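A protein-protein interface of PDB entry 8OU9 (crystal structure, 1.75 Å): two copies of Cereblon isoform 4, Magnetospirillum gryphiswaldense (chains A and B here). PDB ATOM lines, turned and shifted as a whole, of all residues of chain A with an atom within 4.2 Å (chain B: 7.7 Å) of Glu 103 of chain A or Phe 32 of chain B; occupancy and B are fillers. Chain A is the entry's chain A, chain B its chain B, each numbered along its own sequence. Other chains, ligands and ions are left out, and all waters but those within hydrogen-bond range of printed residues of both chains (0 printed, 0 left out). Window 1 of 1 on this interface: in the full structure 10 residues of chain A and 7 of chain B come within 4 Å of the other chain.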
ATOM      1  N   ALA A   2       1.261  24.183  20.662  1.00  0.00           N
ATOM      2  CA  ALA A   2       1.024  25.618  20.448  1.00  0.00           C
ATOM      3  C   ALA A   2       0.530  26.254  21.768  1.00  0.00           C
ATOM      4  O   ALA A   2      -0.640  26.528  22.017  1.00  0.00           O
ATOM      5  CB  ALA A   2       0.100  25.870  19.281  1.00  0.00           C
ATOM      6  N   ILE A   4       2.872  28.547  23.733  1.00  0.00           N
ATOM      7  CA  ILE A   4       3.570  29.794  24.112  1.00  0.00           C
ATOM      8  C   ILE A   4       3.309  30.840  23.006  1.00  0.00           C
ATOM      9  O   ILE A   4       3.213  30.483  21.842  1.00  0.00           O
ATOM     10  CB  ILE A   4       5.045  29.456  24.235  1.00  0.00           C
ATOM     11  CG1 ILE A   4       5.260  28.574  25.501  1.00  0.00           C
ATOM     12  CG2 ILE A   4       5.927  30.644  24.273  1.00  0.00           C
ATOM     13  N   PHE A   5       3.133  32.075  23.382  1.00  0.00           N
ATOM     14  CA  PHE A   5       3.055  33.209  22.447  1.00  0.00           C
ATOM     15  C   PHE A   5       4.364  33.993  22.518  1.00  0.00           C
ATOM     16  O   PHE A   5       4.810  34.376  23.586  1.00  0.00           O
ATOM     17  CB  PHE A   5       1.897  34.080  22.713  1.00  0.00           C
ATOM     18  CG  PHE A   5       0.566  33.446  22.519  1.00  0.00           C
ATOM     19  CD1 PHE A   5       0.049  33.228  21.258  1.00  0.00           C
ATOM     20  CD2 PHE A   5      -0.202  33.095  23.611  1.00  0.00           C
ATOM     21  CE1 PHE A   5      -1.227  32.657  21.096  1.00  0.00           C
ATOM     22  CE2 PHE A   5      -1.459  32.523  23.427  1.00  0.00           C
ATOM     23  CZ  PHE A   5      -1.914  32.236  22.187  1.00  0.00           C
ATOM     24  N   ARG A   6       4.909  34.245  21.316  1.00  0.00           N
ATOM     25  CA  ARG A   6       6.106  35.023  21.114  1.00  0.00           C
ATOM     26  C   ARG A   6       5.767  36.241  20.267  1.00  0.00           C
ATOM     27  O   ARG A   6       4.803  36.209  19.525  1.00  0.00           O
ATOM     28  CB  ARG A   6       7.202  34.156  20.434  1.00  0.00           C
ATOM     29  CG  ARG A   6       7.831  33.138  21.380  1.00  0.00           C
ATOM     30  CD  ARG A   6       8.977  32.321  20.724  1.00  0.00           C
ATOM     31  NE  ARG A   6       9.423  31.331  21.720  1.00  0.00           N
ATOM     32  CZ  ARG A   6      10.162  31.598  22.771  1.00  0.00           C
ATOM     33  NH1 ARG A   6      10.598  32.827  22.964  1.00  0.00           N
ATOM     34  NH2 ARG A   6      10.341  30.644  23.645  1.00  0.00           N
ATOM     35  N   ARG A  17      -0.994  30.253  26.225  1.00  0.00           N
ATOM     36  CA  ARG A  17      -2.419  30.040  25.976  1.00  0.00           C
ATOM     37  C   ARG A  17      -3.148  29.856  27.328  1.00  0.00           C
ATOM     38  O   ARG A  17      -4.272  30.286  27.504  1.00  0.00           O
ATOM     39  CB  ARG A  17      -2.638  28.845  25.015  1.00  0.00           C
ATOM     40  CG  ARG A  17      -4.105  28.511  24.748  1.00  0.00           C
ATOM     41  CD  ARG A  17      -4.395  27.732  23.469  1.00  0.00           C
ATOM     42  NE  ARG A  17      -4.206  28.487  22.207  1.00  0.00           N
ATOM     43  CZ  ARG A  17      -5.052  29.357  21.669  1.00  0.00           C
ATOM     44  NH1 ARG A  17      -6.289  29.513  22.137  1.00  0.00           N
ATOM     45  NH2 ARG A  17      -4.716  29.990  20.561  1.00  0.00           N
ATOM     46  N   ALA A 102       3.058  35.169  17.701  1.00  0.00           N
ATOM     47  CA  ALA A 102       3.207  33.865  17.090  1.00  0.00           C
ATOM     48  C   ALA A 102       3.074  32.738  18.085  1.00  0.00           C
ATOM     49  O   ALA A 102       3.626  32.868  19.142  1.00  0.00           O
ATOM     50  CB  ALA A 102       4.538  33.812  16.368  1.00  0.00           C
ATOM     51  N   GLU A 103       2.216  31.750  17.808  1.00  0.00           N
ATOM     52  CA  GLU A 103       1.969  30.684  18.778  1.00  0.00           C
ATOM     53  C   GLU A 103       2.780  29.447  18.461  1.00  0.00           C
ATOM     54  O   GLU A 103       2.938  29.038  17.306  1.00  0.00           O
ATOM     55  CB  GLU A 103       0.473  30.413  18.745  1.00  0.00           C
ATOM     56  CG  GLU A 103       0.030  29.516  19.895  1.00  0.00           C
ATOM     57  CD  GLU A 103      -1.464  29.159  19.951  1.00  0.00           C
ATOM     58  OE1 GLU A 103      -2.266  29.727  19.113  1.00  0.00           O
ATOM     59  OE2 GLU A 103      -1.865  28.441  20.920  1.00  0.00           O
ATOM     60  N   GLY A 104       3.262  28.790  19.504  1.00  0.00           N
ATOM     61  CA  GLY A 104       4.144  27.683  19.251  1.00  0.00           C
ATOM     62  C   GLY A 104       4.544  26.911  20.496  1.00  0.00           C
ATOM     63  O   GLY A 104       3.981  27.088  21.589  1.00  0.00           O
ATOM     64  N   PRO A 105       5.377  25.862  20.266  1.00  0.00           N
ATOM     65  CA  PRO A 105       5.767  24.938  21.340  1.00  0.00           C
ATOM     66  C   PRO A 105       6.577  25.526  22.484  1.00  0.00           C
ATOM     67  O   PRO A 105       7.367  26.442  22.298  1.00  0.00           O
ATOM     68  CB  PRO A 105       6.571  23.821  20.628  1.00  0.00           C
ATOM     69  CG  PRO A 105       7.018  24.496  19.298  1.00  0.00           C
ATOM     70  CD  PRO A 105       5.863  25.405  18.950  1.00  0.00           C
ATOM     71  N   HIS B  29      -3.658  31.622  11.543  1.00  0.00           N
ATOM     72  CA  HIS B  29      -2.835  31.422  12.720  1.00  0.00           C
ATOM     73  C   HIS B  29      -1.408  31.803  12.381  1.00  0.00           C
ATOM     74  O   HIS B  29      -0.813  31.137  11.488  1.00  0.00           O
ATOM     75  CB  HIS B  29      -2.896  29.952  13.051  1.00  0.00           C
ATOM     76  CG  HIS B  29      -4.274  29.515  13.483  1.00  0.00           C
ATOM     77  ND1 HIS B  29      -4.577  29.183  14.779  1.00  0.00           N
ATOM     78  CD2 HIS B  29      -5.386  29.377  12.788  1.00  0.00           C
ATOM     79  CE1 HIS B  29      -5.867  28.882  14.837  1.00  0.00           C
ATOM     80  NE2 HIS B  29      -6.375  29.059  13.678  1.00  0.00           N
ATOM     81  N   VAL B  30      -0.798  32.707  13.191  1.00  0.00           N
ATOM     82  CA  VAL B  30       0.639  32.894  13.152  1.00  0.00           C
ATOM     83  C   VAL B  30       1.308  31.947  14.157  1.00  0.00           C
ATOM     84  O   VAL B  30       0.925  31.988  15.319  1.00  0.00           O
ATOM     85  CB  VAL B  30       1.008  34.351  13.393  1.00  0.00           C
ATOM     86  CG1 VAL B  30       2.504  34.653  13.265  1.00  0.00           C
ATOM     87  CG2 VAL B  30       0.256  35.316  12.431  1.00  0.00           C
ATOM     88  N   VAL B  31       2.280  31.213  13.664  1.00  0.00           N
ATOM     89  CA  VAL B  31       2.828  30.073  14.378  1.00  0.00           C
ATOM     90  C   VAL B  31       4.362  30.092  14.240  1.00  0.00           C
ATOM     91  O   VAL B  31       4.925  30.588  13.275  1.00  0.00           O
ATOM     92  CB  VAL B  31       2.187  28.761  13.959  1.00  0.00           C
ATOM     93  CG1 VAL B  31       0.733  28.663  14.385  1.00  0.00           C
ATOM     94  CG2 VAL B  31       2.430  28.518  12.490  1.00  0.00           C
ATOM     95  N   PHE B  32       5.049  29.439  15.197  1.00  0.00           N
ATOM     96  CA  PHE B  32       6.477  29.164  15.061  1.00  0.00           C
ATOM     97  C   PHE B  32       6.789  27.677  15.370  1.00  0.00           C
ATOM     98  O   PHE B  32       6.100  27.004  16.139  1.00  0.00           O
ATOM     99  CB  PHE B  32       7.318  30.065  15.973  1.00  0.00           C
ATOM    100  CG  PHE B  32       7.103  29.827  17.454  1.00  0.00           C
ATOM    101  CD1 PHE B  32       6.221  30.632  18.154  1.00  0.00           C
ATOM    102  CD2 PHE B  32       7.926  28.953  18.186  1.00  0.00           C
ATOM    103  CE1 PHE B  32       6.030  30.442  19.535  1.00  0.00           C
ATOM    104  CE2 PHE B  32       7.692  28.719  19.533  1.00  0.00           C
ATOM    105  CZ  PHE B  32       6.727  29.474  20.209  1.00  0.00           C
ATOM    106  N   ASN B  33       7.756  27.145  14.632  1.00  0.00           N
ATOM    107  CA  ASN B  33       8.154  25.749  14.759  1.00  0.00           C
ATOM    108  C   ASN B  33       9.344  25.657  15.738  1.00  0.00           C
ATOM    109  O   ASN B  33       9.743  26.672  16.336  1.00  0.00           O
ATOM    110  CB  ASN B  33       8.345  25.144  13.362  1.00  0.00           C
ATOM    111  CG  ASN B  33       9.630  25.567  12.695  1.00  0.00           C
ATOM    112  OD1 ASN B  33      10.502  26.258  13.305  1.00  0.00           O
ATOM    113  ND2 ASN B  33       9.760  25.153  11.443  1.00  0.00           N
ATOM    114  N   PRO B  34       9.784  24.419  16.066  1.00  0.00           N
ATOM    115  CA  PRO B  34      10.856  24.216  17.025  1.00  0.00           C
ATOM    116  C   PRO B  34      12.194  24.832  16.624  1.00  0.00           C
ATOM    117  O   PRO B  34      13.036  25.045  17.535  1.00  0.00           O
ATOM    118  CB  PRO B  34      11.000  22.714  17.210  1.00  0.00           C
ATOM    119  CG  PRO B  34       9.576  22.244  16.833  1.00  0.00           C
ATOM    120  CD  PRO B  34       9.184  23.135  15.653  1.00  0.00           C
ATOM    121  N   ALA B  35      12.373  25.071  15.355  1.00  0.00           N
ATOM    122  CA  ALA B  35      13.571  25.716  14.858  1.00  0.00           C
ATOM    123  C   ALA B  35      13.424  27.254  14.892  1.00  0.00           C
ATOM    124  O   ALA B  35      14.371  27.993  14.500  1.00  0.00           O
ATOM    125  CB  ALA B  35      13.844  25.174  13.494  1.00  0.00           C
ATOM    126  N   GLY B  36      12.277  27.754  15.397  1.00  0.00           N
ATOM    127  CA  GLY B  36      12.001  29.171  15.535  1.00  0.00           C
ATOM    128  C   GLY B  36      11.645  29.843  14.232  1.00  0.00           C
ATOM    129  O   GLY B  36      11.622  31.057  14.162  1.00  0.00           O
ATOM    130  N   MET B  37      11.276  29.094  13.207  1.00  0.00           N
ATOM    131  CA  MET B  37      10.787  29.716  11.982  1.00  0.00           C
ATOM    132  C   MET B  37       9.316  30.073  12.178  1.00  0.00           C
ATOM    133  O   MET B  37       8.545  29.281  12.772  1.00  0.00           O
ATOM    134  CB  MET B  37      10.905  28.739  10.829  1.00  0.00           C
ATOM    135  CG  MET B  37      12.352  28.372  10.542  1.00  0.00           C
ATOM    136  SD  MET B  37      13.290  29.798   9.905  1.00  0.00           S
ATOM    137  CE  MET B  37      12.146  30.480   8.684  1.00  0.00           C
ATOM    138  N   ILE B  38       8.922  31.298  11.773  1.00  0.00           N
ATOM    139  CA  ILE B  38       7.589  31.840  11.928  1.00  0.00           C
ATOM    140  C   ILE B  38       6.862  31.780  10.594  1.00  0.00           C
ATOM    141  O   ILE B  38       7.401  32.116   9.550  1.00  0.00           O
ATOM    142  CB  ILE B  38       7.579  33.246  12.524  1.00  0.00           C
ATOM    143  CG1 ILE B  38       8.119  33.238  13.946  1.00  0.00           C
ATOM    144  CG2 ILE B  38       6.230  33.931  12.449  1.00  0.00           C
ATOM    145  CD1 ILE B  38       8.479  34.591  14.471  1.00  0.00           C
ATOM    146  N   PHE B  39       5.626  31.259  10.638  1.00  0.00           N
ATOM    147  CA  PHE B  39       4.764  31.166   9.455  1.00  0.00           C
ATOM    148  C   PHE B  39       3.360  31.715   9.748  1.00  0.00           C
ATOM    149  O   PHE B  39       2.824  31.644  10.876  1.00  0.00           O
ATOM    150  CB  PHE B  39       4.570  29.703   9.018  1.00  0.00           C
ATOM    151  CG  PHE B  39       5.770  28.854   8.776  1.00  0.00           C
ATOM    152  CD1 PHE B  39       6.408  28.867   7.571  1.00  0.00           C
ATOM    153  CD2 PHE B  39       6.364  28.169   9.832  1.00  0.00           C
ATOM    154  CE1 PHE B  39       7.521  28.081   7.345  1.00  0.00           C
ATOM    155  CE2 PHE B  39       7.522  27.442   9.620  1.00  0.00           C
ATOM    156  CZ  PHE B  39       8.085  27.373   8.376  1.00  0.00           C
ATOM    157  N   ARG B  40       2.746  32.267   8.712  1.00  0.00           N
ATOM    158  CA  ARG B  40       1.374  32.767   8.787  1.00  0.00           C
ATOM    159  C   ARG B  40       0.563  31.749   7.986  1.00  0.00           C
ATOM    160  O   ARG B  40       0.669  31.712   6.774  1.00  0.00           O
ATOM    161  CB  ARG B  40       1.159  34.220   8.306  1.00  0.00           C
ATOM    162  CG  ARG B  40      -0.285  34.690   8.371  1.00  0.00           C
ATOM    163  CD  ARG B  40      -0.259  36.218   8.285  1.00  0.00           C
ATOM    164  NE  ARG B  40       0.262  36.620   6.984  1.00  0.00           N
ATOM    165  CZ  ARG B  40      -0.518  37.048   5.980  1.00  0.00           C
ATOM    166  NH1 ARG B  40      -1.832  37.010   6.110  1.00  0.00           N
ATOM    167  NH2 ARG B  40       0.039  37.368   4.827  1.00  0.00           N
ATOM    168  N   PHE B  60       4.773  18.430  18.235  1.00  0.00           N
ATOM    169  CA  PHE B  60       4.757  19.883  18.034  1.00  0.00           C
ATOM    170  C   PHE B  60       3.614  20.339  17.138  1.00  0.00           C
ATOM    171  O   PHE B  60       3.592  21.485  16.622  1.00  0.00           O
ATOM    172  CB  PHE B  60       6.061  20.344  17.356  1.00  0.00           C
ATOM    173  CG  PHE B  60       7.308  19.940  18.098  1.00  0.00           C
ATOM    174  CD1 PHE B  60       7.507  20.378  19.394  1.00  0.00           C
ATOM    175  CD2 PHE B  60       8.242  19.096  17.512  1.00  0.00           C
ATOM    176  CE1 PHE B  60       8.647  19.997  20.092  1.00  0.00           C
ATOM    177  CE2 PHE B  60       9.392  18.733  18.207  1.00  0.00           C
ATOM    178  CZ  PHE B  60       9.565  19.153  19.502  1.00  0.00           C
ATOM    179  N   TRP B  62       0.673  22.172  15.789  1.00  0.00           N
ATOM    180  CA  TRP B  62       0.069  23.432  16.196  1.00  0.00           C
ATOM    181  C   TRP B  62      -1.408  23.257  16.546  1.00  0.00           C
ATOM    182  O   TRP B  62      -2.008  24.161  17.126  1.00  0.00           O
ATOM    183  CB  TRP B  62       0.214  24.521  15.121  1.00  0.00           C
ATOM    184  CG  TRP B  62       1.635  24.912  14.915  1.00  0.00           C
ATOM    185  CD1 TRP B  62       2.527  25.269  15.914  1.00  0.00           C
ATOM    186  CD2 TRP B  62       2.309  25.052  13.684  1.00  0.00           C
ATOM    187  NE1 TRP B  62       3.722  25.597  15.327  1.00  0.00           N
ATOM    188  CE2 TRP B  62       3.617  25.471  13.975  1.00  0.00           C
ATOM    189  CE3 TRP B  62       1.971  24.789  12.344  1.00  0.00           C
ATOM    190  CZ2 TRP B  62       4.554  25.715  12.974  1.00  0.00           C
ATOM    191  CZ3 TRP B  62       2.898  25.006  11.365  1.00  0.00           C
ATOM    192  CH2 TRP B  62       4.188  25.499  11.684  1.00  0.00           C
ATOM    193  N   PHE B  63      -2.011  22.149  16.157  1.00  0.00           N
ATOM    194  CA  PHE B  63      -3.439  21.950  16.378  1.00  0.00           C
ATOM    195  C   PHE B  63      -3.697  20.675  17.172  1.00  0.00           C
ATOM    196  O   PHE B  63      -3.368  19.589  16.724  1.00  0.00           O
ATOM    197  CB  PHE B  63      -4.156  21.840  15.029  1.00  0.00           C
ATOM    198  CG  PHE B  63      -4.013  23.098  14.204  1.00  0.00           C
ATOM    199  CD1 PHE B  63      -4.787  24.220  14.464  1.00  0.00           C
ATOM    200  CD2 PHE B  63      -3.058  23.182  13.208  1.00  0.00           C
ATOM    201  CE1 PHE B  63      -4.607  25.407  13.754  1.00  0.00           C
ATOM    202  CE2 PHE B  63      -2.922  24.352  12.492  1.00  0.00           C
ATOM    203  CZ  PHE B  63      -3.693  25.454  12.733  1.00  0.00           C
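The backbone carbonyl oxygen (O) of Val 31 of chain B sits at hydrogen-bond distance from the backbone NH (N) of Phe 39 of chain B (2.8 Å).
OE2 of Glu 103 of chain A sits close to O of Ala 2 of chain A, 2.5 Å away.
O of Phe 32 of chain B sits at hydrogen-bond distance from NE1 of Trp 62 of chain B, at 2.9 Å.
The guanidinium group (NE) of Arg 17 of chain A lies within salt-bridge range of the side-chain carboxylate (OE2) of Glu 103 of chain A (2.7 Å).
The backbone NH of Ala 102 of chain A is in hydrogen-bond range of the backbone carbonyl oxygen of Arg 6 of chain A.
N of Ile 4 of chain A is in hydrogen-bond range of O of Gly 104 of chain A, 2.8 Å away.
Of chain B, only Val 30, Val 31 and Phe 32 come within 4 Å of Glu 103 of chain A.
Phe 32 of chain B touches six residues of chain A.
Of chain B, only Val 30 and Phe 32 come within 4 Å of Ala 102 of chain A.
Printed residues of chain B within 4 Å of Ala 2 of chain A: Trp 62 (3.5 Å).
Of the printed residues of chain A, Phe 60 of chain B touches Pro 105 (3.8 Å).
Of the printed residues of chain A, Val 31 of chain B touches Glu 103 (3.1 Å).
Printed residues of chain B within 4 Å of Pro 105 of chain A: Phe 32 and Phe 60.
Gly 36 of chain B touches none of the printed residues of chain A.
Ala 2 of chain A touches Trp 62 of chain B.
Ile 4 of chain A touches Phe 32 of chain B (O to CE1, 3.6 Å).
NE of Arg 6 of chain A touches CZ of Phe 32 of chain B, at 3.6 Å.
O of Val 30 of chain B touches CA of Ala 102 of chain A, 3.4 Å away.
O of Ala 102 of chain A touches CE1 of Phe 32 of chain B (3.4 Å).
Glu 103 of chain A touches Val 31 of chain B (O to CA, 3.1 Å).
CE1 of Phe 32 of chain B touches N of Gly 104 of chain A (3.2 Å).
Phe 32 of chain B touches Pro 105 of chain A.
CB of Pro 105 of chain A touches CD1 of Phe 60 of chain B (3.8 Å).
The backbone NH (N) of Phe 32 of chain B lies within hydrogen-bond range of the backbone carbonyl oxygen (O) of Glu 103 of chain A (3.0 Å).
The backbone NH of Glu 103 of chain A lies within hydrogen-bond range of the backbone carbonyl oxygen of Val 30 of chain B, 2.8 Å away.
No position is printed for both chains.
Of the 11 pairs that touch across the chains among the printed residues, none has its exchanged pair printed and touching as well.
Hydrophobic or aromatic side chains of chain A within 4 Å of the printed part of chain B: Ala 2, Ala 102 and Pro 105.
Of the 15 printed residues of chain B, 5 touch a printed residue of chain A.
Hydrophobic or aromatic side chains of chain B that line the printed part of chain A: Val 30, Val 31, Phe 32 and Phe 60.
Among the printed residues, no Asp or Glu carboxylate lies within 4 Å of a Lys or Arg side-chain nitrogen of the other chain.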
